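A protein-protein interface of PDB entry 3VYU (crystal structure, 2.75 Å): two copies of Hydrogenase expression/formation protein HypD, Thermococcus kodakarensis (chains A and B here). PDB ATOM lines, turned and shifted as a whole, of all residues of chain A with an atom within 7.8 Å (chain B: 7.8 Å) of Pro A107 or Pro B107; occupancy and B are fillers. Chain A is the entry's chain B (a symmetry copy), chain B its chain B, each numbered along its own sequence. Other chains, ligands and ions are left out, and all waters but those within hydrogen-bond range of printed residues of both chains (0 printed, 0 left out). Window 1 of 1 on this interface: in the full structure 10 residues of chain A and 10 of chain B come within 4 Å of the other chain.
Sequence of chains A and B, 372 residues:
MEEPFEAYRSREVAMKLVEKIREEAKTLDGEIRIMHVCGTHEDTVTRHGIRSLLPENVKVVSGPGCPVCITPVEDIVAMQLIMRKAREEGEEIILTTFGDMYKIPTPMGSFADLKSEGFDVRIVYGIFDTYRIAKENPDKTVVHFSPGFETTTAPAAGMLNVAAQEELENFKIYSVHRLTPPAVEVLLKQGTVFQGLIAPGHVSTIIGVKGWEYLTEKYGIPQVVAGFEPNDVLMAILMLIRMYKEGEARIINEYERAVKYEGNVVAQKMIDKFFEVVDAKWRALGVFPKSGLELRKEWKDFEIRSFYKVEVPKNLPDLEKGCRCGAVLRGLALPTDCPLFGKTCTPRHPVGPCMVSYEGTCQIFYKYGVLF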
ATOM      1  N   VAL A  73     -34.453  19.052   7.371  1.00  0.00           N
ATOM      2  CA  VAL A  73     -33.405  19.690   6.607  1.00  0.00           C
ATOM      3  C   VAL A  73     -33.245  18.948   5.298  1.00  0.00           C
ATOM      4  O   VAL A  73     -33.033  19.542   4.256  1.00  0.00           O
ATOM      5  CB  VAL A  73     -32.065  19.636   7.349  1.00  0.00           C
ATOM      6  CG1 VAL A  73     -32.202  20.276   8.707  1.00  0.00           C
ATOM      7  CG2 VAL A  73     -31.602  18.209   7.490  1.00  0.00           C
ATOM      8  N   GLU A  74     -33.350  17.630   5.364  1.00  0.00           N
ATOM      9  CA  GLU A  74     -33.168  16.803   4.184  1.00  0.00           C
ATOM     10  C   GLU A  74     -33.956  17.311   2.979  1.00  0.00           C
ATOM     11  O   GLU A  74     -33.466  17.282   1.851  1.00  0.00           O
ATOM     12  CB  GLU A  74     -33.554  15.354   4.501  1.00  0.00           C
ATOM     13  CG  GLU A  74     -32.872  14.796   5.754  1.00  0.00           C
ATOM     14  CD  GLU A  74     -33.729  14.924   7.005  1.00  0.00           C
ATOM     15  OE1 GLU A  74     -34.760  14.224   7.081  1.00  0.00           O
ATOM     16  OE2 GLU A  74     -33.378  15.715   7.909  1.00  0.00           O
ATOM     17  N   VAL A  77     -32.644  21.016   1.888  1.00  0.00           N
ATOM     18  CA  VAL A  77     -31.401  20.830   1.141  1.00  0.00           C
ATOM     19  C   VAL A  77     -31.768  20.242  -0.225  1.00  0.00           C
ATOM     20  O   VAL A  77     -31.306  20.721  -1.262  1.00  0.00           O
ATOM     21  CB  VAL A  77     -30.419  19.868   1.904  1.00  0.00           C
ATOM     22  CG1 VAL A  77     -29.210  19.540   1.041  1.00  0.00           C
ATOM     23  CG2 VAL A  77     -29.939  20.524   3.196  1.00  0.00           C
ATOM     24  N   GLN A  80     -32.900  22.745  -2.661  1.00  0.00           N
ATOM     25  CA  GLN A  80     -31.821  23.594  -3.163  1.00  0.00           C
ATOM     26  C   GLN A  80     -31.044  22.827  -4.233  1.00  0.00           C
ATOM     27  O   GLN A  80     -30.526  23.421  -5.183  1.00  0.00           O
ATOM     28  CB  GLN A  80     -30.870  24.007  -2.030  1.00  0.00           C
ATOM     29  CG  GLN A  80     -31.536  24.717  -0.850  1.00  0.00           C
ATOM     30  CD  GLN A  80     -30.528  25.290   0.136  1.00  0.00           C
ATOM     31  OE1 GLN A  80     -29.387  24.837   0.205  1.00  0.00           O
ATOM     32  NE2 GLN A  80     -30.951  26.280   0.913  1.00  0.00           N
ATOM     33  N   ILE A 104     -34.791  29.666   7.364  1.00  0.00           N
ATOM     34  CA  ILE A 104     -34.426  28.462   8.113  1.00  0.00           C
ATOM     35  C   ILE A 104     -33.038  27.962   7.744  1.00  0.00           C
ATOM     36  O   ILE A 104     -32.700  27.826   6.567  1.00  0.00           O
ATOM     37  CB  ILE A 104     -35.439  27.312   7.912  1.00  0.00           C
ATOM     38  CG1 ILE A 104     -36.755  27.649   8.604  1.00  0.00           C
ATOM     39  CG2 ILE A 104     -34.906  26.028   8.529  1.00  0.00           C
ATOM     40  CD1 ILE A 104     -36.627  27.780  10.100  1.00  0.00           C
ATOM     41  N   PRO A 105     -32.211  27.681   8.760  1.00  0.00           N
ATOM     42  CA  PRO A 105     -30.842  27.199   8.581  1.00  0.00           C
ATOM     43  C   PRO A 105     -30.687  25.700   8.367  1.00  0.00           C
ATOM     44  O   PRO A 105     -31.466  24.894   8.876  1.00  0.00           O
ATOM     45  CB  PRO A 105     -30.162  27.658   9.863  1.00  0.00           C
ATOM     46  CG  PRO A 105     -31.229  27.419  10.869  1.00  0.00           C
ATOM     47  CD  PRO A 105     -32.473  27.974  10.182  1.00  0.00           C
ATOM     48  N   THR A 106     -29.662  25.347   7.600  1.00  0.00           N
ATOM     49  CA  THR A 106     -29.318  23.963   7.310  1.00  0.00           C
ATOM     50  C   THR A 106     -27.808  23.975   7.120  1.00  0.00           C
ATOM     51  O   THR A 106     -27.233  24.997   6.738  1.00  0.00           O
ATOM     52  CB  THR A 106     -29.967  23.456   6.011  1.00  0.00           C
ATOM     53  OG1 THR A 106     -29.313  24.054   4.886  1.00  0.00           O
ATOM     54  CG2 THR A 106     -31.445  23.806   5.979  1.00  0.00           C
ATOM     55  N   PRO A 107     -27.141  22.844   7.378  1.00  0.00           N
ATOM     56  CA  PRO A 107     -25.687  22.822   7.207  1.00  0.00           C
ATOM     57  C   PRO A 107     -25.233  23.247   5.811  1.00  0.00           C
ATOM     58  O   PRO A 107     -24.080  23.625   5.617  1.00  0.00           O
ATOM     59  CB  PRO A 107     -25.328  21.374   7.536  1.00  0.00           C
ATOM     60  CG  PRO A 107     -26.558  20.620   7.135  1.00  0.00           C
ATOM     61  CD  PRO A 107     -27.659  21.497   7.669  1.00  0.00           C
ATOM     62  N   MET A 108     -26.147  23.202   4.848  1.00  0.00           N
ATOM     63  CA  MET A 108     -25.830  23.576   3.474  1.00  0.00           C
ATOM     64  C   MET A 108     -26.246  24.997   3.136  1.00  0.00           C
ATOM     65  O   MET A 108     -26.191  25.401   1.975  1.00  0.00           O
ATOM     66  CB  MET A 108     -26.518  22.623   2.502  1.00  0.00           C
ATOM     67  CG  MET A 108     -26.156  21.170   2.709  1.00  0.00           C
ATOM     68  SD  MET A 108     -24.416  20.843   2.409  1.00  0.00           S
ATOM     69  CE  MET A 108     -24.498  20.025   0.818  1.00  0.00           C
ATOM     70  N   GLY A 109     -26.669  25.751   4.144  1.00  0.00           N
ATOM     71  CA  GLY A 109     -27.096  27.120   3.907  1.00  0.00           C
ATOM     72  C   GLY A 109     -28.605  27.222   3.762  1.00  0.00           C
ATOM     73  O   GLY A 109     -29.282  26.212   3.565  1.00  0.00           O
ATOM     74  N   SER A 110     -29.134  28.440   3.849  1.00  0.00           N
ATOM     75  CA  SER A 110     -30.574  28.655   3.744  1.00  0.00           C
ATOM     76  C   SER A 110     -31.010  29.091   2.353  1.00  0.00           C
ATOM     77  O   SER A 110     -30.182  29.406   1.498  1.00  0.00           O
ATOM     78  CB  SER A 110     -31.029  29.710   4.752  1.00  0.00           C
ATOM     79  OG  SER A 110     -30.505  30.984   4.418  1.00  0.00           O
ATOM     80  N   ARG A 283     -38.313  17.196  11.864  1.00  0.00           N
ATOM     81  CA  ARG A 283     -37.014  17.693  12.270  1.00  0.00           C
ATOM     82  C   ARG A 283     -36.838  17.741  13.776  1.00  0.00           C
ATOM     83  O   ARG A 283     -37.687  18.268  14.496  1.00  0.00           O
ATOM     84  CB  ARG A 283     -36.784  19.081  11.688  1.00  0.00           C
ATOM     85  CG  ARG A 283     -35.377  19.604  11.894  1.00  0.00           C
ATOM     86  CD  ARG A 283     -35.229  20.954  11.241  1.00  0.00           C
ATOM     87  NE  ARG A 283     -33.858  21.440  11.272  1.00  0.00           N
ATOM     88  CZ  ARG A 283     -33.463  22.543  10.650  1.00  0.00           C
ATOM     89  NH1 ARG A 283     -34.341  23.258   9.960  1.00  0.00           N
ATOM     90  NH2 ARG A 283     -32.196  22.926  10.707  1.00  0.00           N
ATOM     91  N   PRO A 313     -27.005  14.667   0.623  1.00  0.00           N
ATOM     92  CA  PRO A 313     -25.893  14.126   1.411  1.00  0.00           C
ATOM     93  C   PRO A 313     -26.345  13.487   2.723  1.00  0.00           C
ATOM     94  O   PRO A 313     -27.250  13.988   3.389  1.00  0.00           O
ATOM     95  CB  PRO A 313     -24.991  15.345   1.622  1.00  0.00           C
ATOM     96  CG  PRO A 313     -25.948  16.494   1.576  1.00  0.00           C
ATOM     97  CD  PRO A 313     -26.848  16.119   0.427  1.00  0.00           C
ATOM     98  N   ASN A 315     -25.805  12.110   6.675  1.00  0.00           N
ATOM     99  CA  ASN A 315     -25.162  12.599   7.886  1.00  0.00           C
ATOM    100  C   ASN A 315     -25.295  14.110   8.072  1.00  0.00           C
ATOM    101  O   ASN A 315     -24.371  14.766   8.552  1.00  0.00           O
ATOM    102  CB  ASN A 315     -23.683  12.196   7.905  1.00  0.00           C
ATOM    103  CG  ASN A 315     -23.485  10.697   7.755  1.00  0.00           C
ATOM    104  OD1 ASN A 315     -23.971   9.909   8.567  1.00  0.00           O
ATOM    105  ND2 ASN A 315     -22.770  10.296   6.709  1.00  0.00           N
ATOM    106  N   LEU A 316     -26.445  14.656   7.686  1.00  0.00           N
ATOM    107  CA  LEU A 316     -26.712  16.084   7.849  1.00  0.00           C
ATOM    108  C   LEU A 316     -27.420  16.288   9.179  1.00  0.00           C
ATOM    109  O   LEU A 316     -28.598  15.964   9.321  1.00  0.00           O
ATOM    110  CB  LEU A 316     -27.620  16.609   6.738  1.00  0.00           C
ATOM    111  CG  LEU A 316     -27.079  16.716   5.316  1.00  0.00           C
ATOM    112  CD1 LEU A 316     -28.128  17.379   4.428  1.00  0.00           C
ATOM    113  CD2 LEU A 316     -25.796  17.530   5.317  1.00  0.00           C
ATOM    114  N   PRO A 317     -26.713  16.833  10.176  1.00  0.00           N
ATOM    115  CA  PRO A 317     -27.335  17.055  11.484  1.00  0.00           C
ATOM    116  C   PRO A 317     -28.586  17.937  11.430  1.00  0.00           C
ATOM    117  O   PRO A 317     -28.628  18.929  10.699  1.00  0.00           O
ATOM    118  CB  PRO A 317     -26.203  17.680  12.298  1.00  0.00           C
ATOM    119  CG  PRO A 317     -25.391  18.388  11.257  1.00  0.00           C
ATOM    120  CD  PRO A 317     -25.348  17.381  10.139  1.00  0.00           C
ATOM    121  N   ASP A 318     -29.596  17.551  12.207  1.00  0.00           N
ATOM    122  CA  ASP A 318     -30.873  18.259  12.298  1.00  0.00           C
ATOM    123  C   ASP A 318     -30.733  19.627  12.952  1.00  0.00           C
ATOM    124  O   ASP A 318     -31.332  20.599  12.495  1.00  0.00           O
ATOM    125  CB  ASP A 318     -31.876  17.423  13.103  1.00  0.00           C
ATOM    126  CG  ASP A 318     -32.644  16.431  12.244  1.00  0.00           C
ATOM    127  OD1 ASP A 318     -32.086  15.941  11.236  1.00  0.00           O
ATOM    128  OD2 ASP A 318     -33.808  16.131  12.586  1.00  0.00           O
ATOM    129  N   LEU A 319     -29.951  19.692  14.028  1.00  0.00           N
ATOM    130  CA  LEU A 319     -29.729  20.937  14.762  1.00  0.00           C
ATOM    131  C   LEU A 319     -28.248  21.109  15.084  1.00  0.00           C
ATOM    132  O   LEU A 319     -27.497  20.136  15.097  1.00  0.00           O
ATOM    133  CB  LEU A 319     -30.515  20.916  16.072  1.00  0.00           C
ATOM    134  CG  LEU A 319     -32.011  20.606  15.988  1.00  0.00           C
ATOM    135  CD1 LEU A 319     -32.582  20.429  17.387  1.00  0.00           C
ATOM    136  CD2 LEU A 319     -32.722  21.730  15.253  1.00  0.00           C
ATOM    137  N   GLU A 320     -27.828  22.343  15.343  1.00  0.00           N
ATOM    138  CA  GLU A 320     -26.435  22.598  15.691  1.00  0.00           C
ATOM    139  C   GLU A 320     -26.189  22.252  17.158  1.00  0.00           C
ATOM    140  O   GLU A 320     -27.103  22.322  17.980  1.00  0.00           O
ATOM    141  CB  GLU A 320     -26.070  24.064  15.425  1.00  0.00           C
ATOM    142  CG  GLU A 320     -25.768  24.356  13.963  1.00  0.00           C
ATOM    143  CD  GLU A 320     -24.566  23.572  13.455  1.00  0.00           C
ATOM    144  OE1 GLU A 320     -24.420  23.424  12.220  1.00  0.00           O
ATOM    145  OE2 GLU A 320     -23.761  23.110  14.293  1.00  0.00           O
ATOM    146  N   VAL B  73     -12.659  22.455   4.522  1.00  0.00           N
ATOM    147  CA  VAL B  73     -13.705  21.623   5.073  1.00  0.00           C
ATOM    148  C   VAL B  73     -13.840  20.388   4.211  1.00  0.00           C
ATOM    149  O   VAL B  73     -14.045  19.292   4.704  1.00  0.00           O
ATOM    150  CB  VAL B  73     -15.053  22.352   5.071  1.00  0.00           C
ATOM    151  CG1 VAL B  73     -14.941  23.646   5.836  1.00  0.00           C
ATOM    152  CG2 VAL B  73     -15.501  22.619   3.658  1.00  0.00           C
ATOM    153  N   GLU B  74     -13.720  20.576   2.907  1.00  0.00           N
ATOM    154  CA  GLU B  74     -13.878  19.476   1.972  1.00  0.00           C
ATOM    155  C   GLU B  74     -13.080  18.239   2.377  1.00  0.00           C
ATOM    156  O   GLU B  74     -13.556  17.113   2.237  1.00  0.00           O
ATOM    157  CB  GLU B  74     -13.479  19.931   0.564  1.00  0.00           C
ATOM    158  CG  GLU B  74     -14.170  21.222   0.116  1.00  0.00           C
ATOM    159  CD  GLU B  74     -13.330  22.465   0.369  1.00  0.00           C
ATOM    160  OE1 GLU B  74     -12.292  22.618  -0.308  1.00  0.00           O
ATOM    161  OE2 GLU B  74     -13.702  23.288   1.236  1.00  0.00           O
ATOM    162  N   VAL B  77     -14.421  16.794   5.947  1.00  0.00           N
ATOM    163  CA  VAL B  77     -15.653  16.053   5.677  1.00  0.00           C
ATOM    164  C   VAL B  77     -15.261  14.752   4.971  1.00  0.00           C
ATOM    165  O   VAL B  77     -15.715  13.670   5.345  1.00  0.00           O
ATOM    166  CB  VAL B  77     -16.633  16.890   4.778  1.00  0.00           C
ATOM    167  CG1 VAL B  77     -17.827  16.047   4.356  1.00  0.00           C
ATOM    168  CG2 VAL B  77     -17.137  18.110   5.544  1.00  0.00           C
ATOM    169  N   GLN B  80     -14.128  12.107   7.252  1.00  0.00           N
ATOM    170  CA  GLN B  80     -15.209  11.516   8.036  1.00  0.00           C
ATOM    171  C   GLN B  80     -15.964  10.513   7.164  1.00  0.00           C
ATOM    172  O   GLN B  80     -16.477   9.507   7.661  1.00  0.00           O
ATOM    173  CB  GLN B  80     -16.180  12.595   8.541  1.00  0.00           C
ATOM    174  CG  GLN B  80     -15.537  13.712   9.365  1.00  0.00           C
ATOM    175  CD  GLN B  80     -16.564  14.629  10.014  1.00  0.00           C
ATOM    176  OE1 GLN B  80     -17.700  14.727   9.554  1.00  0.00           O
ATOM    177  NE2 GLN B  80     -16.162  15.316  11.077  1.00  0.00           N
ATOM    178  N   ILE B 104     -12.444  21.469  15.094  1.00  0.00           N
ATOM    179  CA  ILE B 104     -12.805  22.323  13.960  1.00  0.00           C
ATOM    180  C   ILE B 104     -14.182  21.985  13.410  1.00  0.00           C
ATOM    181  O   ILE B 104     -14.503  20.822  13.162  1.00  0.00           O
ATOM    182  CB  ILE B 104     -11.776  22.240  12.808  1.00  0.00           C
ATOM    183  CG1 ILE B 104     -10.473  22.914  13.225  1.00  0.00           C
ATOM    184  CG2 ILE B 104     -12.302  22.967  11.581  1.00  0.00           C
ATOM    185  CD1 ILE B 104     -10.621  24.389  13.492  1.00  0.00           C
ATOM    186  N   PRO B 105     -15.018  23.013  13.214  1.00  0.00           N
ATOM    187  CA  PRO B 105     -16.379  22.864  12.700  1.00  0.00           C
ATOM    188  C   PRO B 105     -16.514  22.788  11.185  1.00  0.00           C
ATOM    189  O   PRO B 105     -15.732  23.378  10.440  1.00  0.00           O
ATOM    190  CB  PRO B 105     -17.081  24.089  13.267  1.00  0.00           C
ATOM    191  CG  PRO B 105     -16.024  25.126  13.136  1.00  0.00           C
ATOM    192  CD  PRO B 105     -14.778  24.404  13.640  1.00  0.00           C
ATOM    193  N   THR B 106     -17.526  22.045  10.751  1.00  0.00           N
ATOM    194  CA  THR B 106     -17.850  21.881   9.341  1.00  0.00           C
ATOM    195  C   THR B 106     -19.357  21.673   9.317  1.00  0.00           C
ATOM    196  O   THR B 106     -19.938  21.191  10.291  1.00  0.00           O
ATOM    197  CB  THR B 106     -17.178  20.641   8.725  1.00  0.00           C
ATOM    198  OG1 THR B 106     -17.825  19.459   9.207  1.00  0.00           O
ATOM    199  CG2 THR B 106     -15.704  20.595   9.089  1.00  0.00           C
ATOM    200  N   PRO B 107     -20.014  22.026   8.206  1.00  0.00           N
ATOM    201  CA  PRO B 107     -21.465  21.841   8.149  1.00  0.00           C
ATOM    202  C   PRO B 107     -21.907  20.407   8.438  1.00  0.00           C
ATOM    203  O   PRO B 107     -23.061  20.165   8.782  1.00  0.00           O
ATOM    204  CB  PRO B 107     -21.812  22.299   6.734  1.00  0.00           C
ATOM    205  CG  PRO B 107     -20.568  21.984   5.961  1.00  0.00           C
ATOM    206  CD  PRO B 107     -19.484  22.447   6.898  1.00  0.00           C
ATOM    207  N   MET B 108     -20.980  19.463   8.316  1.00  0.00           N
ATOM    208  CA  MET B 108     -21.284  18.057   8.556  1.00  0.00           C
ATOM    209  C   MET B 108     -20.880  17.594   9.945  1.00  0.00           C
ATOM    210  O   MET B 108     -20.925  16.400  10.240  1.00  0.00           O
ATOM    211  CB  MET B 108     -20.572  17.185   7.527  1.00  0.00           C
ATOM    212  CG  MET B 108     -20.920  17.522   6.094  1.00  0.00           C
ATOM    213  SD  MET B 108     -22.652  17.233   5.719  1.00  0.00           S
ATOM    214  CE  MET B 108     -22.541  15.726   4.758  1.00  0.00           C
ATOM    215  N   GLY B 109     -20.479  18.532  10.795  1.00  0.00           N
ATOM    216  CA  GLY B 109     -20.064  18.174  12.141  1.00  0.00           C
ATOM    217  C   GLY B 109     -18.555  18.038  12.249  1.00  0.00           C
ATOM    218  O   GLY B 109     -17.864  17.943  11.234  1.00  0.00           O
ATOM    219  N   SER B 110     -18.041  18.018  13.476  1.00  0.00           N
ATOM    220  CA  SER B 110     -16.602  17.909  13.698  1.00  0.00           C
ATOM    221  C   SER B 110     -16.154  16.490  14.009  1.00  0.00           C
ATOM    222  O   SER B 110     -16.975  15.600  14.233  1.00  0.00           O
ATOM    223  CB  SER B 110     -16.173  18.821  14.848  1.00  0.00           C
ATOM    224  OG  SER B 110     -16.708  18.365  16.079  1.00  0.00           O
ATOM    225  N   ARG B 283      -8.836  27.146   3.139  1.00  0.00           N
ATOM    226  CA  ARG B 283     -10.145  27.489   3.655  1.00  0.00           C
ATOM    227  C   ARG B 283     -10.341  28.982   3.840  1.00  0.00           C
ATOM    228  O   ARG B 283      -9.507  29.659   4.442  1.00  0.00           O
ATOM    229  CB  ARG B 283     -10.384  26.778   4.981  1.00  0.00           C
ATOM    230  CG  ARG B 283     -11.799  26.918   5.502  1.00  0.00           C
ATOM    231  CD  ARG B 283     -11.955  26.141   6.784  1.00  0.00           C
ATOM    232  NE  ARG B 283     -13.331  26.111   7.254  1.00  0.00           N
ATOM    233  CZ  ARG B 283     -13.731  25.385   8.289  1.00  0.00           C
ATOM    234  NH1 ARG B 283     -12.853  24.642   8.948  1.00  0.00           N
ATOM    235  NH2 ARG B 283     -15.003  25.392   8.660  1.00  0.00           N
ATOM    236  N   PRO B 313     -19.970  16.058  -0.562  1.00  0.00           N
ATOM    237  CA  PRO B 313     -21.085  16.879  -1.042  1.00  0.00           C
ATOM    238  C   PRO B 313     -20.643  18.250  -1.551  1.00  0.00           C
ATOM    239  O   PRO B 313     -19.752  18.878  -0.979  1.00  0.00           O
ATOM    240  CB  PRO B 313     -22.004  16.965   0.180  1.00  0.00           C
ATOM    241  CG  PRO B 313     -21.059  16.825   1.332  1.00  0.00           C
ATOM    242  CD  PRO B 313     -20.141  15.726   0.863  1.00  0.00           C
ATOM    243  N   ASN B 315     -21.216  22.306  -2.564  1.00  0.00           N
ATOM    244  CA  ASN B 315     -21.880  23.459  -1.973  1.00  0.00           C
ATOM    245  C   ASN B 315     -21.768  23.506  -0.450  1.00  0.00           C
ATOM    246  O   ASN B 315     -22.705  23.912   0.237  1.00  0.00           O
ATOM    247  CB  ASN B 315     -23.355  23.498  -2.391  1.00  0.00           C
ATOM    248  CG  ASN B 315     -23.534  23.485  -3.900  1.00  0.00           C
ATOM    249  OD1 ASN B 315     -23.049  24.373  -4.603  1.00  0.00           O
ATOM    250  ND2 ASN B 315     -24.231  22.472  -4.405  1.00  0.00           N
ATOM    251  N   LEU B 316     -20.620  23.084   0.073  1.00  0.00           N
ATOM    252  CA  LEU B 316     -20.371  23.117   1.513  1.00  0.00           C
ATOM    253  C   LEU B 316     -19.683  24.431   1.848  1.00  0.00           C
ATOM    254  O   LEU B 316     -18.502  24.615   1.553  1.00  0.00           O
ATOM    255  CB  LEU B 316     -19.455  21.973   1.945  1.00  0.00           C
ATOM    256  CG  LEU B 316     -19.979  20.541   1.913  1.00  0.00           C
ATOM    257  CD1 LEU B 316     -18.927  19.608   2.504  1.00  0.00           C
ATOM    258  CD2 LEU B 316     -21.272  20.452   2.707  1.00  0.00           C
ATOM    259  N   PRO B 317     -20.408  25.364   2.474  1.00  0.00           N
ATOM    260  CA  PRO B 317     -19.806  26.653   2.824  1.00  0.00           C
ATOM    261  C   PRO B 317     -18.564  26.532   3.714  1.00  0.00           C
ATOM    262  O   PRO B 317     -18.524  25.713   4.634  1.00  0.00           O
ATOM    263  CB  PRO B 317     -20.955  27.393   3.508  1.00  0.00           C
ATOM    264  CG  PRO B 317     -21.762  26.282   4.106  1.00  0.00           C
ATOM    265  CD  PRO B 317     -21.779  25.261   2.999  1.00  0.00           C
ATOM    266  N   ASP B 318     -17.560  27.354   3.413  1.00  0.00           N
ATOM    267  CA  ASP B 318     -16.292  27.393   4.143  1.00  0.00           C
ATOM    268  C   ASP B 318     -16.456  27.916   5.564  1.00  0.00           C
ATOM    269  O   ASP B 318     -15.863  27.378   6.497  1.00  0.00           O
ATOM    270  CB  ASP B 318     -15.290  28.284   3.398  1.00  0.00           C
ATOM    271  CG  ASP B 318     -14.500  27.529   2.341  1.00  0.00           C
ATOM    272  OD1 ASP B 318     -15.039  26.565   1.753  1.00  0.00           O
ATOM    273  OD2 ASP B 318     -13.337  27.912   2.088  1.00  0.00           O
ATOM    274  N   LEU B 319     -17.252  28.972   5.719  1.00  0.00           N
ATOM    275  CA  LEU B 319     -17.498  29.585   7.023  1.00  0.00           C
ATOM    276  C   LEU B 319     -18.985  29.872   7.205  1.00  0.00           C
ATOM    277  O   LEU B 319     -19.725  29.967   6.228  1.00  0.00           O
ATOM    278  CB  LEU B 319     -16.728  30.900   7.133  1.00  0.00           C
ATOM    279  CG  LEU B 319     -15.229  30.863   6.836  1.00  0.00           C
ATOM    280  CD1 LEU B 319     -14.673  32.279   6.797  1.00  0.00           C
ATOM    281  CD2 LEU B 319     -14.521  30.035   7.896  1.00  0.00           C
ATOM    282  N   GLU B 320     -19.423  30.011   8.452  1.00  0.00           N
ATOM    283  CA  GLU B 320     -20.823  30.318   8.720  1.00  0.00           C
ATOM    284  C   GLU B 320     -21.083  31.808   8.509  1.00  0.00           C
ATOM    285  O   GLU B 320     -20.181  32.630   8.667  1.00  0.00           O
ATOM    286  CB  GLU B 320     -21.201  29.913  10.151  1.00  0.00           C
ATOM    287  CG  GLU B 320     -21.488  28.427  10.302  1.00  0.00           C
ATOM    288  CD  GLU B 320     -22.674  27.979   9.460  1.00  0.00           C
ATOM    289  OE1 GLU B 320     -22.803  26.763   9.196  1.00  0.00           O
ATOM    290  OE2 GLU B 320     -23.484  28.848   9.067  1.00  0.00           O
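Of chain B, only Pro B107 (2.9 Å) and Pro B317 (3.8 Å) come within 4 Å of Pro A107.
Pro B107 touches just these residues of chain A: Pro A107 and Pro A317.
Printed residues of chain B within 4 Å of Pro A313: Met B108 (3.998 Å) and Pro B313 (3.7 Å).
Printed residues of chain A within 4 Å of Met B108: Pro A313 (3.998 Å) and Leu A316 (3.2 Å).
Of the printed residues of chain A, Pro B317 touches Pro A107.
Of the printed residues of chain B, Met A108 touches Pro B313 and Leu B316.
Of the printed residues of chain A, Pro B313 touches Met A108 and Pro A313.
Pro A105 touches none of the printed residues of chain B.
The nearest residue of chain A that does not touch Pro B107 is Met A108 (4.8 Å).
The nearest printed residue of chain B that does not touch Pro A313 is Leu B316 (6.2 Å).
Among the printed residues, merely in contact across the chains: Pro A107 with Pro B107, Met A108 with Leu B316, Leu A316 with Met B108, Pro A313 with Pro B313, Pro A317 with Pro B107, Pro A107 with Pro B317, Pro A313 with Met B108 and Met A108 with Pro B313.
Hydrophobic or aromatic side chains of chain B within 4 Å of the printed part of chain A: Pro B107, Met B108, Pro B313, Leu B316 and Pro B317.
Hydrophobic or aromatic side chains of chain A that line the printed part of chain B: Pro A107, Met A108, Pro A313, Leu A316 and Pro A317.
Among the printed residues, no Asp or Glu carboxylate lies within 4 Å of a Lys or Arg side-chain nitrogen of the other chain.
The side-chain hydroxyl of Thr B106 sits close to the backbone NH of Met B108, at 3.3 Å.
The backbone NH of Met A108 sits close to the side-chain hydroxyl of Thr A106.
Pro A107 touches Pro B317, and with the chains exchanged Pro A317 touches Pro B107.
Met A108 touches Pro B313, and with the chains exchanged Pro A313 touches Met B108.
Met A108 touches Leu B316, and with the chains exchanged Leu A316 touches Met B108.
Pro B313 touches its own counterpart, Pro A313.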
